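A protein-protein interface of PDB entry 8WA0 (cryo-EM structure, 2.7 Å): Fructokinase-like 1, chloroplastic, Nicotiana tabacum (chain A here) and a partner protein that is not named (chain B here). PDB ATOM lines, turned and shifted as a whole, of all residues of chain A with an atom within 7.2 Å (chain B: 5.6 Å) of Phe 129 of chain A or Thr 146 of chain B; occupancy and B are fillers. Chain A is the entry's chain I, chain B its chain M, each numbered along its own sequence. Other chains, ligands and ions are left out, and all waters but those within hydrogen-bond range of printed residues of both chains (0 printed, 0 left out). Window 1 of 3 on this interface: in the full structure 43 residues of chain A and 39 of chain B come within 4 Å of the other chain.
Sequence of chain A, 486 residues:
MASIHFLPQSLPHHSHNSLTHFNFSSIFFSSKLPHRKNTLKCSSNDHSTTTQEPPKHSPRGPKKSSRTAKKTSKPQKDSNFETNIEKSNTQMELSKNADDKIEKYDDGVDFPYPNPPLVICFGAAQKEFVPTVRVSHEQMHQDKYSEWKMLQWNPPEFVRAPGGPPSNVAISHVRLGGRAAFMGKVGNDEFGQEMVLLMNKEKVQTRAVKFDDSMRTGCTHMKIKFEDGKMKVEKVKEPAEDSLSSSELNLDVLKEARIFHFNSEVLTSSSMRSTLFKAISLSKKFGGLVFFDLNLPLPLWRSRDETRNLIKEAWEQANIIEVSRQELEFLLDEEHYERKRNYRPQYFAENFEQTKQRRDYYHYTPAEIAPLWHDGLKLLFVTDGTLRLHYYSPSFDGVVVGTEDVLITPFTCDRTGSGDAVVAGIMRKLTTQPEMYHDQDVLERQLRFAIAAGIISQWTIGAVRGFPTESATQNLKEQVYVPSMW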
ATOM      1  N   GLN A 126      -3.110   6.516   1.617  1.00  0.00           N
ATOM      2  CA  GLN A 126      -2.236   5.389   1.530  1.00  0.00           C
ATOM      3  C   GLN A 126      -0.830   5.952   1.471  1.00  0.00           C
ATOM      4  O   GLN A 126      -0.649   7.009   0.899  1.00  0.00           O
ATOM      5  CB  GLN A 126      -2.635   4.595   0.323  1.00  0.00           C
ATOM      6  CG  GLN A 126      -3.787   3.644   0.558  1.00  0.00           C
ATOM      7  CD  GLN A 126      -4.583   3.398  -0.696  1.00  0.00           C
ATOM      8  OE1 GLN A 126      -4.390   4.066  -1.706  1.00  0.00           O
ATOM      9  NE2 GLN A 126      -5.499   2.445  -0.636  1.00  0.00           N
ATOM     10  N   LYS A 127       0.173   5.318   2.076  1.00  0.00           N
ATOM     11  CA  LYS A 127       1.495   5.939   2.163  1.00  0.00           C
ATOM     12  C   LYS A 127       2.339   6.221   0.941  1.00  0.00           C
ATOM     13  O   LYS A 127       2.726   7.377   0.760  1.00  0.00           O
ATOM     14  CB  LYS A 127       2.329   5.270   3.231  1.00  0.00           C
ATOM     15  CG  LYS A 127       3.789   5.676   3.266  1.00  0.00           C
ATOM     16  CD  LYS A 127       4.007   6.929   4.089  1.00  0.00           C
ATOM     17  CE  LYS A 127       4.009   6.601   5.566  1.00  0.00           C
ATOM     18  NZ  LYS A 127       5.057   5.596   5.884  1.00  0.00           N
ATOM     19  N   GLU A 128       2.596   5.239   0.089  1.00  0.00           N
ATOM     20  CA  GLU A 128       3.307   5.475  -1.164  1.00  0.00           C
ATOM     21  C   GLU A 128       2.775   4.442  -2.101  1.00  0.00           C
ATOM     22  O   GLU A 128       3.427   3.444  -2.335  1.00  0.00           O
ATOM     23  CB  GLU A 128       4.797   5.252  -1.008  1.00  0.00           C
ATOM     24  CG  GLU A 128       5.567   6.286  -0.200  1.00  0.00           C
ATOM     25  CD  GLU A 128       5.871   7.547  -0.983  1.00  0.00           C
ATOM     26  OE1 GLU A 128       5.935   7.480  -2.227  1.00  0.00           O
ATOM     27  OE2 GLU A 128       6.060   8.607  -0.353  1.00  0.00           O
ATOM     28  N   PHE A 129       1.604   4.665  -2.661  1.00  0.00           N
ATOM     29  CA  PHE A 129       0.972   3.663  -3.484  1.00  0.00           C
ATOM     30  C   PHE A 129       0.869   4.173  -4.892  1.00  0.00           C
ATOM     31  O   PHE A 129       0.468   5.298  -5.103  1.00  0.00           O
ATOM     32  CB  PHE A 129      -0.417   3.465  -2.927  1.00  0.00           C
ATOM     33  CG  PHE A 129      -1.036   2.152  -3.239  1.00  0.00           C
ATOM     34  CD1 PHE A 129      -0.372   0.982  -2.973  1.00  0.00           C
ATOM     35  CD2 PHE A 129      -2.319   2.098  -3.736  1.00  0.00           C
ATOM     36  CE1 PHE A 129      -0.962  -0.231  -3.237  1.00  0.00           C
ATOM     37  CE2 PHE A 129      -2.921   0.893  -3.998  1.00  0.00           C
ATOM     38  CZ  PHE A 129      -2.241  -0.275  -3.739  1.00  0.00           C
ATOM     39  N   VAL A 130       1.252   3.363  -5.864  1.00  0.00           N
ATOM     40  CA  VAL A 130       1.103   3.754  -7.241  1.00  0.00           C
ATOM     41  C   VAL A 130      -0.059   2.970  -7.768  1.00  0.00           C
ATOM     42  O   VAL A 130       0.016   1.765  -7.878  1.00  0.00           O
ATOM     43  CB  VAL A 130       2.332   3.355  -8.048  1.00  0.00           C
ATOM     44  CG1 VAL A 130       2.205   3.824  -9.486  1.00  0.00           C
ATOM     45  CG2 VAL A 130       3.587   3.920  -7.414  1.00  0.00           C
ATOM     46  N   PRO A 131      -1.149   3.645  -8.096  1.00  0.00           N
ATOM     47  CA  PRO A 131      -2.331   2.982  -8.630  1.00  0.00           C
ATOM     48  C   PRO A 131      -2.227   2.337  -9.999  1.00  0.00           C
ATOM     49  O   PRO A 131      -2.776   1.267 -10.148  1.00  0.00           O
ATOM     50  CB  PRO A 131      -3.350   4.096  -8.662  1.00  0.00           C
ATOM     51  CG  PRO A 131      -2.564   5.351  -8.759  1.00  0.00           C
ATOM     52  CD  PRO A 131      -1.343   5.094  -7.945  1.00  0.00           C
ATOM     53  N   THR A 132      -1.551   2.932 -10.974  1.00  0.00           N
ATOM     54  CA  THR A 132      -1.545   2.394 -12.342  1.00  0.00           C
ATOM     55  C   THR A 132      -0.515   1.338 -12.620  1.00  0.00           C
ATOM     56  O   THR A 132       0.670   1.592 -12.530  1.00  0.00           O
ATOM     57  CB  THR A 132      -1.298   3.506 -13.371  1.00  0.00           C
ATOM     58  OG1 THR A 132       0.057   3.951 -13.293  1.00  0.00           O
ATOM     59  CG2 THR A 132      -2.205   4.687 -13.114  1.00  0.00           C
ATOM     60  N   GLY A 163       0.930   9.363 -11.020  1.00  0.00           N
ATOM     61  CA  GLY A 163       0.085   9.965 -10.025  1.00  0.00           C
ATOM     62  C   GLY A 163      -0.087   9.133  -8.790  1.00  0.00           C
ATOM     63  O   GLY A 163       0.532   8.086  -8.671  1.00  0.00           O
ATOM     64  N   GLY A 164      -0.909   9.563  -7.865  1.00  0.00           N
ATOM     65  CA  GLY A 164      -1.012   8.859  -6.611  1.00  0.00           C
ATOM     66  C   GLY A 164      -2.217   9.041  -5.753  1.00  0.00           C
ATOM     67  O   GLY A 164      -3.247   9.466  -6.235  1.00  0.00           O
ATOM     68  N   PRO A 165      -2.107   8.727  -4.478  1.00  0.00           N
ATOM     69  CA  PRO A 165      -3.203   8.836  -3.533  1.00  0.00           C
ATOM     70  C   PRO A 165      -3.692  10.237  -3.313  1.00  0.00           C
ATOM     71  O   PRO A 165      -2.926  11.170  -3.484  1.00  0.00           O
ATOM     72  CB  PRO A 165      -2.567   8.357  -2.268  1.00  0.00           C
ATOM     73  CG  PRO A 165      -1.469   7.456  -2.677  1.00  0.00           C
ATOM     74  CD  PRO A 165      -0.908   8.145  -3.868  1.00  0.00           C
ATOM     75  N   ASN A 168      -1.661  12.880  -1.062  1.00  0.00           N
ATOM     76  CA  ASN A 168      -0.525  13.581  -1.608  1.00  0.00           C
ATOM     77  C   ASN A 168      -0.847  14.880  -2.274  1.00  0.00           C
ATOM     78  O   ASN A 168      -0.104  15.829  -2.132  1.00  0.00           O
ATOM     79  CB  ASN A 168       0.268  12.664  -2.529  1.00  0.00           C
ATOM     80  CG  ASN A 168       0.877  11.485  -1.815  1.00  0.00           C
ATOM     81  OD1 ASN A 168       0.777  11.351  -0.601  1.00  0.00           O
ATOM     82  ND2 ASN A 168       1.520  10.619  -2.573  1.00  0.00           N
ATOM     83  N   GLU A 265     -10.313   5.380  -7.774  1.00  0.00           N
ATOM     84  CA  GLU A 265     -10.247   4.256  -6.870  1.00  0.00           C
ATOM     85  C   GLU A 265     -11.500   4.118  -6.070  1.00  0.00           C
ATOM     86  O   GLU A 265     -11.880   3.025  -5.686  1.00  0.00           O
ATOM     87  CB  GLU A 265      -9.063   4.392  -5.948  1.00  0.00           C
ATOM     88  CG  GLU A 265      -8.831   3.244  -4.993  1.00  0.00           C
ATOM     89  CD  GLU A 265      -8.421   3.726  -3.617  1.00  0.00           C
ATOM     90  OE1 GLU A 265      -8.939   4.773  -3.178  1.00  0.00           O
ATOM     91  OE2 GLU A 265      -7.587   3.057  -2.972  1.00  0.00           O
ATOM     92  N   THR A 416       7.866   9.264  -8.681  1.00  0.00           N
ATOM     93  CA  THR A 416       6.641   8.916  -7.961  1.00  0.00           C
ATOM     94  C   THR A 416       5.518   9.928  -7.669  1.00  0.00           C
ATOM     95  O   THR A 416       4.360   9.552  -7.754  1.00  0.00           O
ATOM     96  CB  THR A 416       6.963   8.090  -6.707  1.00  0.00           C
ATOM     97  OG1 THR A 416       5.750   7.620  -6.113  1.00  0.00           O
ATOM     98  CG2 THR A 416       7.720   8.916  -5.704  1.00  0.00           C
ATOM     99  N   ASP A 420       0.814  14.245  -8.998  1.00  0.00           N
ATOM    100  CA  ASP A 420       0.113  14.915  -7.947  1.00  0.00           C
ATOM    101  C   ASP A 420       0.448  16.353  -7.927  1.00  0.00           C
ATOM    102  O   ASP A 420      -0.417  17.176  -7.703  1.00  0.00           O
ATOM    103  CB  ASP A 420       0.521  14.280  -6.654  1.00  0.00           C
ATOM    104  CG  ASP A 420       0.193  12.811  -6.607  1.00  0.00           C
ATOM    105  OD1 ASP A 420      -0.815  12.413  -7.225  1.00  0.00           O
ATOM    106  OD2 ASP A 420       0.934  12.051  -5.949  1.00  0.00           O
ATOM    107  N   ILE B  94       3.600 -13.102   0.720  1.00  0.00           N
ATOM    108  CA  ILE B  94       3.848 -12.958  -0.708  1.00  0.00           C
ATOM    109  C   ILE B  94       3.896 -11.501  -1.107  1.00  0.00           C
ATOM    110  O   ILE B  94       2.989 -10.778  -0.796  1.00  0.00           O
ATOM    111  CB  ILE B  94       2.746 -13.616  -1.543  1.00  0.00           C
ATOM    112  CG1 ILE B  94       2.427 -15.009  -1.046  1.00  0.00           C
ATOM    113  CG2 ILE B  94       3.109 -13.651  -3.015  1.00  0.00           C
ATOM    114  CD1 ILE B  94       1.358 -15.672  -1.876  1.00  0.00           C
ATOM    115  N   ASP B  95       4.913 -11.079  -1.842  1.00  0.00           N
ATOM    116  CA  ASP B  95       5.042  -9.697  -2.271  1.00  0.00           C
ATOM    117  C   ASP B  95       4.914  -9.541  -3.764  1.00  0.00           C
ATOM    118  O   ASP B  95       5.536 -10.271  -4.506  1.00  0.00           O
ATOM    119  CB  ASP B  95       6.402  -9.190  -1.851  1.00  0.00           C
ATOM    120  CG  ASP B  95       6.636  -7.749  -2.229  1.00  0.00           C
ATOM    121  OD1 ASP B  95       5.685  -6.947  -2.168  1.00  0.00           O
ATOM    122  OD2 ASP B  95       7.786  -7.411  -2.574  1.00  0.00           O
ATOM    123  N   PHE B  96       4.141  -8.572  -4.214  1.00  0.00           N
ATOM    124  CA  PHE B  96       3.986  -8.323  -5.627  1.00  0.00           C
ATOM    125  C   PHE B  96       4.803  -7.106  -5.958  1.00  0.00           C
ATOM    126  O   PHE B  96       4.674  -6.098  -5.302  1.00  0.00           O
ATOM    127  CB  PHE B  96       2.529  -8.071  -5.951  1.00  0.00           C
ATOM    128  CG  PHE B  96       1.670  -9.295  -5.926  1.00  0.00           C
ATOM    129  CD1 PHE B  96       1.102  -9.735  -4.749  1.00  0.00           C
ATOM    130  CD2 PHE B  96       1.403  -9.985  -7.089  1.00  0.00           C
ATOM    131  CE1 PHE B  96       0.306 -10.857  -4.729  1.00  0.00           C
ATOM    132  CE2 PHE B  96       0.604 -11.106  -7.077  1.00  0.00           C
ATOM    133  CZ  PHE B  96       0.054 -11.542  -5.895  1.00  0.00           C
ATOM    134  N   PRO B 103       8.700   3.113  -5.359  1.00  0.00           N
ATOM    135  CA  PRO B 103       8.466   2.732  -3.977  1.00  0.00           C
ATOM    136  C   PRO B 103       8.924   1.331  -3.652  1.00  0.00           C
ATOM    137  O   PRO B 103       9.307   1.070  -2.530  1.00  0.00           O
ATOM    138  CB  PRO B 103       6.971   2.844  -3.869  1.00  0.00           C
ATOM    139  CG  PRO B 103       6.650   4.015  -4.707  1.00  0.00           C
ATOM    140  CD  PRO B 103       7.564   3.892  -5.886  1.00  0.00           C
ATOM    141  N   VAL B 141      -5.334  -7.078  -6.839  1.00  0.00           N
ATOM    142  CA  VAL B 141      -4.273  -6.191  -6.449  1.00  0.00           C
ATOM    143  C   VAL B 141      -4.583  -4.902  -7.155  1.00  0.00           C
ATOM    144  O   VAL B 141      -4.752  -4.889  -8.361  1.00  0.00           O
ATOM    145  CB  VAL B 141      -2.920  -6.738  -6.922  1.00  0.00           C
ATOM    146  CG1 VAL B 141      -1.811  -5.732  -6.693  1.00  0.00           C
ATOM    147  CG2 VAL B 141      -2.601  -8.047  -6.230  1.00  0.00           C
ATOM    148  N   ARG B 142      -4.648  -3.801  -6.432  1.00  0.00           N
ATOM    149  CA  ARG B 142      -5.014  -2.548  -7.051  1.00  0.00           C
ATOM    150  C   ARG B 142      -3.848  -1.605  -7.310  1.00  0.00           C
ATOM    151  O   ARG B 142      -3.984  -0.666  -8.064  1.00  0.00           O
ATOM    152  CB  ARG B 142      -6.072  -1.863  -6.211  1.00  0.00           C
ATOM    153  CG  ARG B 142      -7.352  -2.657  -6.040  1.00  0.00           C
ATOM    154  CD  ARG B 142      -8.498  -1.761  -5.599  1.00  0.00           C
ATOM    155  NE  ARG B 142      -8.724  -1.781  -4.157  1.00  0.00           N
ATOM    156  CZ  ARG B 142      -8.237  -0.886  -3.303  1.00  0.00           C
ATOM    157  NH1 ARG B 142      -7.486   0.111  -3.738  1.00  0.00           N
ATOM    158  NH2 ARG B 142      -8.504  -0.987  -2.013  1.00  0.00           N
ATOM    159  N   GLY B 143      -2.705  -1.843  -6.696  1.00  0.00           N
ATOM    160  CA  GLY B 143      -1.558  -0.976  -6.856  1.00  0.00           C
ATOM    161  C   GLY B 143      -0.307  -1.724  -6.520  1.00  0.00           C
ATOM    162  O   GLY B 143      -0.378  -2.769  -5.912  1.00  0.00           O
ATOM    163  N   LEU B 144       0.851  -1.210  -6.899  1.00  0.00           N
ATOM    164  CA  LEU B 144       2.069  -1.992  -6.732  1.00  0.00           C
ATOM    165  C   LEU B 144       2.721  -2.419  -5.453  1.00  0.00           C
ATOM    166  O   LEU B 144       3.167  -3.551  -5.357  1.00  0.00           O
ATOM    167  CB  LEU B 144       3.122  -1.626  -7.732  1.00  0.00           C
ATOM    168  CG  LEU B 144       3.008  -2.545  -8.932  1.00  0.00           C
ATOM    169  CD1 LEU B 144       4.107  -2.211  -9.904  1.00  0.00           C
ATOM    170  CD2 LEU B 144       3.078  -4.001  -8.517  1.00  0.00           C
ATOM    171  N   PRO B 145       2.803  -1.550  -4.451  1.00  0.00           N
ATOM    172  CA  PRO B 145       3.444  -2.136  -3.263  1.00  0.00           C
ATOM    173  C   PRO B 145       2.414  -2.919  -2.438  1.00  0.00           C
ATOM    174  O   PRO B 145       1.832  -2.339  -1.540  1.00  0.00           O
ATOM    175  CB  PRO B 145       4.009  -0.926  -2.532  1.00  0.00           C
ATOM    176  CG  PRO B 145       3.996   0.188  -3.523  1.00  0.00           C
ATOM    177  CD  PRO B 145       2.838  -0.082  -4.428  1.00  0.00           C
ATOM    178  N   THR B 146       2.180  -4.201  -2.742  1.00  0.00           N
ATOM    179  CA  THR B 146       1.142  -4.988  -2.060  1.00  0.00           C
ATOM    180  C   THR B 146       1.600  -6.311  -1.500  1.00  0.00           C
ATOM    181  O   THR B 146       2.264  -7.062  -2.185  1.00  0.00           O
ATOM    182  CB  THR B 146      -0.041  -5.265  -2.995  1.00  0.00           C
ATOM    183  OG1 THR B 146      -0.546  -4.028  -3.504  1.00  0.00           O
ATOM    184  CG2 THR B 146      -1.161  -5.976  -2.276  1.00  0.00           C
ATOM    185  N   LEU B 147       1.220  -6.617  -0.267  1.00  0.00           N
ATOM    186  CA  LEU B 147       1.641  -7.845   0.388  1.00  0.00           C
ATOM    187  C   LEU B 147       0.469  -8.671   0.867  1.00  0.00           C
ATOM    188  O   LEU B 147      -0.489  -8.115   1.368  1.00  0.00           O
ATOM    189  CB  LEU B 147       2.507  -7.507   1.595  1.00  0.00           C
ATOM    190  CG  LEU B 147       3.988  -7.158   1.470  1.00  0.00           C
ATOM    191  CD1 LEU B 147       4.188  -5.761   0.917  1.00  0.00           C
ATOM    192  CD2 LEU B 147       4.619  -7.246   2.845  1.00  0.00           C
ATOM    193  N   TYR B 148       0.529  -9.989   0.719  1.00  0.00           N
ATOM    194  CA  TYR B 148      -0.519 -10.875   1.205  1.00  0.00           C
ATOM    195  C   TYR B 148       0.044 -11.725   2.277  1.00  0.00           C
ATOM    196  O   TYR B 148       1.025 -12.385   2.061  1.00  0.00           O
ATOM    197  CB  TYR B 148      -1.089 -11.752   0.104  1.00  0.00           C
ATOM    198  CG  TYR B 148      -2.031 -11.060  -0.820  1.00  0.00           C
ATOM    199  CD1 TYR B 148      -1.572 -10.081  -1.674  1.00  0.00           C
ATOM    200  CD2 TYR B 148      -3.378 -11.371  -0.835  1.00  0.00           C
ATOM    201  CE1 TYR B 148      -2.422  -9.424  -2.518  1.00  0.00           C
ATOM    202  CE2 TYR B 148      -4.241 -10.719  -1.683  1.00  0.00           C
ATOM    203  CZ  TYR B 148      -3.744  -9.748  -2.521  1.00  0.00           C
ATOM    204  OH  TYR B 148      -4.547  -9.050  -3.375  1.00  0.00           O
ATOM    205  N   ARG B 160      -4.624  -8.520   3.211  1.00  0.00           N
ATOM    206  CA  ARG B 160      -3.922  -7.791   2.167  1.00  0.00           C
ATOM    207  C   ARG B 160      -3.581  -6.422   2.613  1.00  0.00           C
ATOM    208  O   ARG B 160      -4.446  -5.691   3.043  1.00  0.00           O
ATOM    209  CB  ARG B 160      -4.777  -7.652   0.930  1.00  0.00           C
ATOM    210  CG  ARG B 160      -4.149  -6.893  -0.215  1.00  0.00           C
ATOM    211  CD  ARG B 160      -5.172  -6.522  -1.273  1.00  0.00           C
ATOM    212  NE  ARG B 160      -6.114  -5.530  -0.780  1.00  0.00           N
ATOM    213  CZ  ARG B 160      -7.125  -5.035  -1.482  1.00  0.00           C
ATOM    214  NH1 ARG B 160      -7.346  -5.451  -2.709  1.00  0.00           N
ATOM    215  NH2 ARG B 160      -7.928  -4.141  -0.939  1.00  0.00           N
ATOM    216  N   THR B 161      -2.327  -6.047   2.524  1.00  0.00           N
ATOM    217  CA  THR B 161      -1.895  -4.718   2.880  1.00  0.00           C
ATOM    218  C   THR B 161      -1.396  -3.934   1.698  1.00  0.00           C
ATOM    219  O   THR B 161      -0.562  -4.396   0.960  1.00  0.00           O
ATOM    220  CB  THR B 161      -0.823  -4.783   3.937  1.00  0.00           C
ATOM    221  OG1 THR B 161      -1.270  -5.618   5.009  1.00  0.00           O
ATOM    222  CG2 THR B 161      -0.546  -3.411   4.483  1.00  0.00           C
ATOM    223  N   GLU B 162      -1.921  -2.747   1.504  1.00  0.00           N
ATOM    224  CA  GLU B 162      -1.514  -1.905   0.414  1.00  0.00           C
ATOM    225  C   GLU B 162      -0.726  -0.678   0.793  1.00  0.00           C
ATOM    226  O   GLU B 162      -1.144   0.094   1.627  1.00  0.00           O
ATOM    227  CB  GLU B 162      -2.716  -1.523  -0.389  1.00  0.00           C
ATOM    228  CG  GLU B 162      -4.000  -1.382   0.405  1.00  0.00           C
ATOM    229  CD  GLU B 162      -5.212  -1.241  -0.494  1.00  0.00           C
ATOM    230  OE1 GLU B 162      -5.071  -1.440  -1.720  1.00  0.00           O
ATOM    231  OE2 GLU B 162      -6.306  -0.938   0.025  1.00  0.00           O
ATOM    232  N   GLY B 163       0.432  -0.495   0.182  1.00  0.00           N
ATOM    233  CA  GLY B 163       1.294   0.618   0.496  1.00  0.00           C
ATOM    234  C   GLY B 163       2.550   0.260   1.203  1.00  0.00           C
ATOM    235  O   GLY B 163       2.740  -0.880   1.574  1.00  0.00           O
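The backbone carbonyl oxygen of Val 130 of chain A is in hydrogen-bond range of the backbone NH of Leu 144 of chain B (3.2 Å).
The side-chain carboxylate (OE2) of Glu 265 of chain A is in salt-bridge range of the guanidinium group (NH1) of Arg 142 of chain B (3.0 Å).
The backbone carbonyl oxygen (O) of Arg 142 of chain B lies close to the backbone carbonyl oxygen (O) of Pro 131 of chain A, at 3.1 Å.
OE2 of Glu 265 of chain A is in hydrogen-bond range of NE2 of Gln 126 of chain A, at 3.2 Å.
The backbone carbonyl oxygen of Thr 146 of chain B is in hydrogen-bond range of the backbone NH of Phe 96 of chain B (3.1 Å).
The guanidinium group (NH2) of Arg 142 of chain B is in salt-bridge range of the side-chain carboxylate (OE2) of Glu 162 of chain B (3.0 Å).
The backbone carbonyl oxygen (O) of Gly 143 of chain B is in hydrogen-bond range of the side-chain hydroxyl (OG1) of Thr 146 of chain B.
O of Pro 145 of chain B lies within hydrogen-bond range of N of Gly 163 of chain B, 2.9 Å away.
NH2 of Arg 160 of chain B lies within salt-bridge range of OE2 of Glu 162 of chain B (3.7 Å).
Glu 162 of chain B touches Gln 126 of chain A (OE2 to NE2, 3.5 Å).
Glu 128 of chain A touches Pro 103 of chain B.
Pro 145 of chain B touches Glu 128 of chain A.
CZ of Phe 129 of chain A touches CA of Gly 143 of chain B (3.3 Å).
Pro 145 of chain B touches Phe 129 of chain A (CD to CD1, 3.7 Å).
Phe 129 of chain A touches Thr 146 of chain B (CE1 to OG1, 3.8 Å).
Glu 162 of chain B touches Phe 129 of chain A.
Phe 129 of chain A touches Gly 163 of chain B (CD1 to N, 3.6 Å).
CA of Gly 143 of chain B touches O of Val 130 of chain A (3.3 Å).
CG of Pro 103 of chain B touches OG1 of Thr 416 of chain A (3.97 Å).
Phe 129 of chain A touches just these residues of chain B: Gly 143, Pro 145, Thr 146, Glu 162 and Gly 163.
Of chain A, only Phe 129 comes within 4 Å of Thr 146 of chain B.
Of the printed residues of chain A, Pro 103 of chain B touches Glu 128 (3.9 Å) and Thr 416 (3.97 Å).
Printed residues of chain B within 4 Å of Gln 126 of chain A: Glu 162.
Of the printed residues of chain B, Val 130 of chain A touches Gly 143 and Leu 144.
Printed residues of chain A within 4 Å of Gly 163 of chain B: Phe 129.
Printed residues of chain A within 4 Å of Leu 144 of chain B: Val 130 (3.2 Å).
The nearest printed residue of chain A that does not touch Thr 146 of chain B is Val 130 of chain A (7.3 Å).
Of the 14 printed residues of chain A, 7 touch a printed residue of chain B.
Along chain A the printed residues that touch a printed residue of chain B span positions 126 to 416.
Printed residues of chain B that touch a printed residue of chain A: Pro 103, Arg 142, Gly 143, Leu 144, Pro 145, Thr 146, Glu 162 and Gly 163.
Hydrophobic or aromatic side chains of chain B within 4 Å of the printed part of chain A: Pro 103 and Pro 145.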
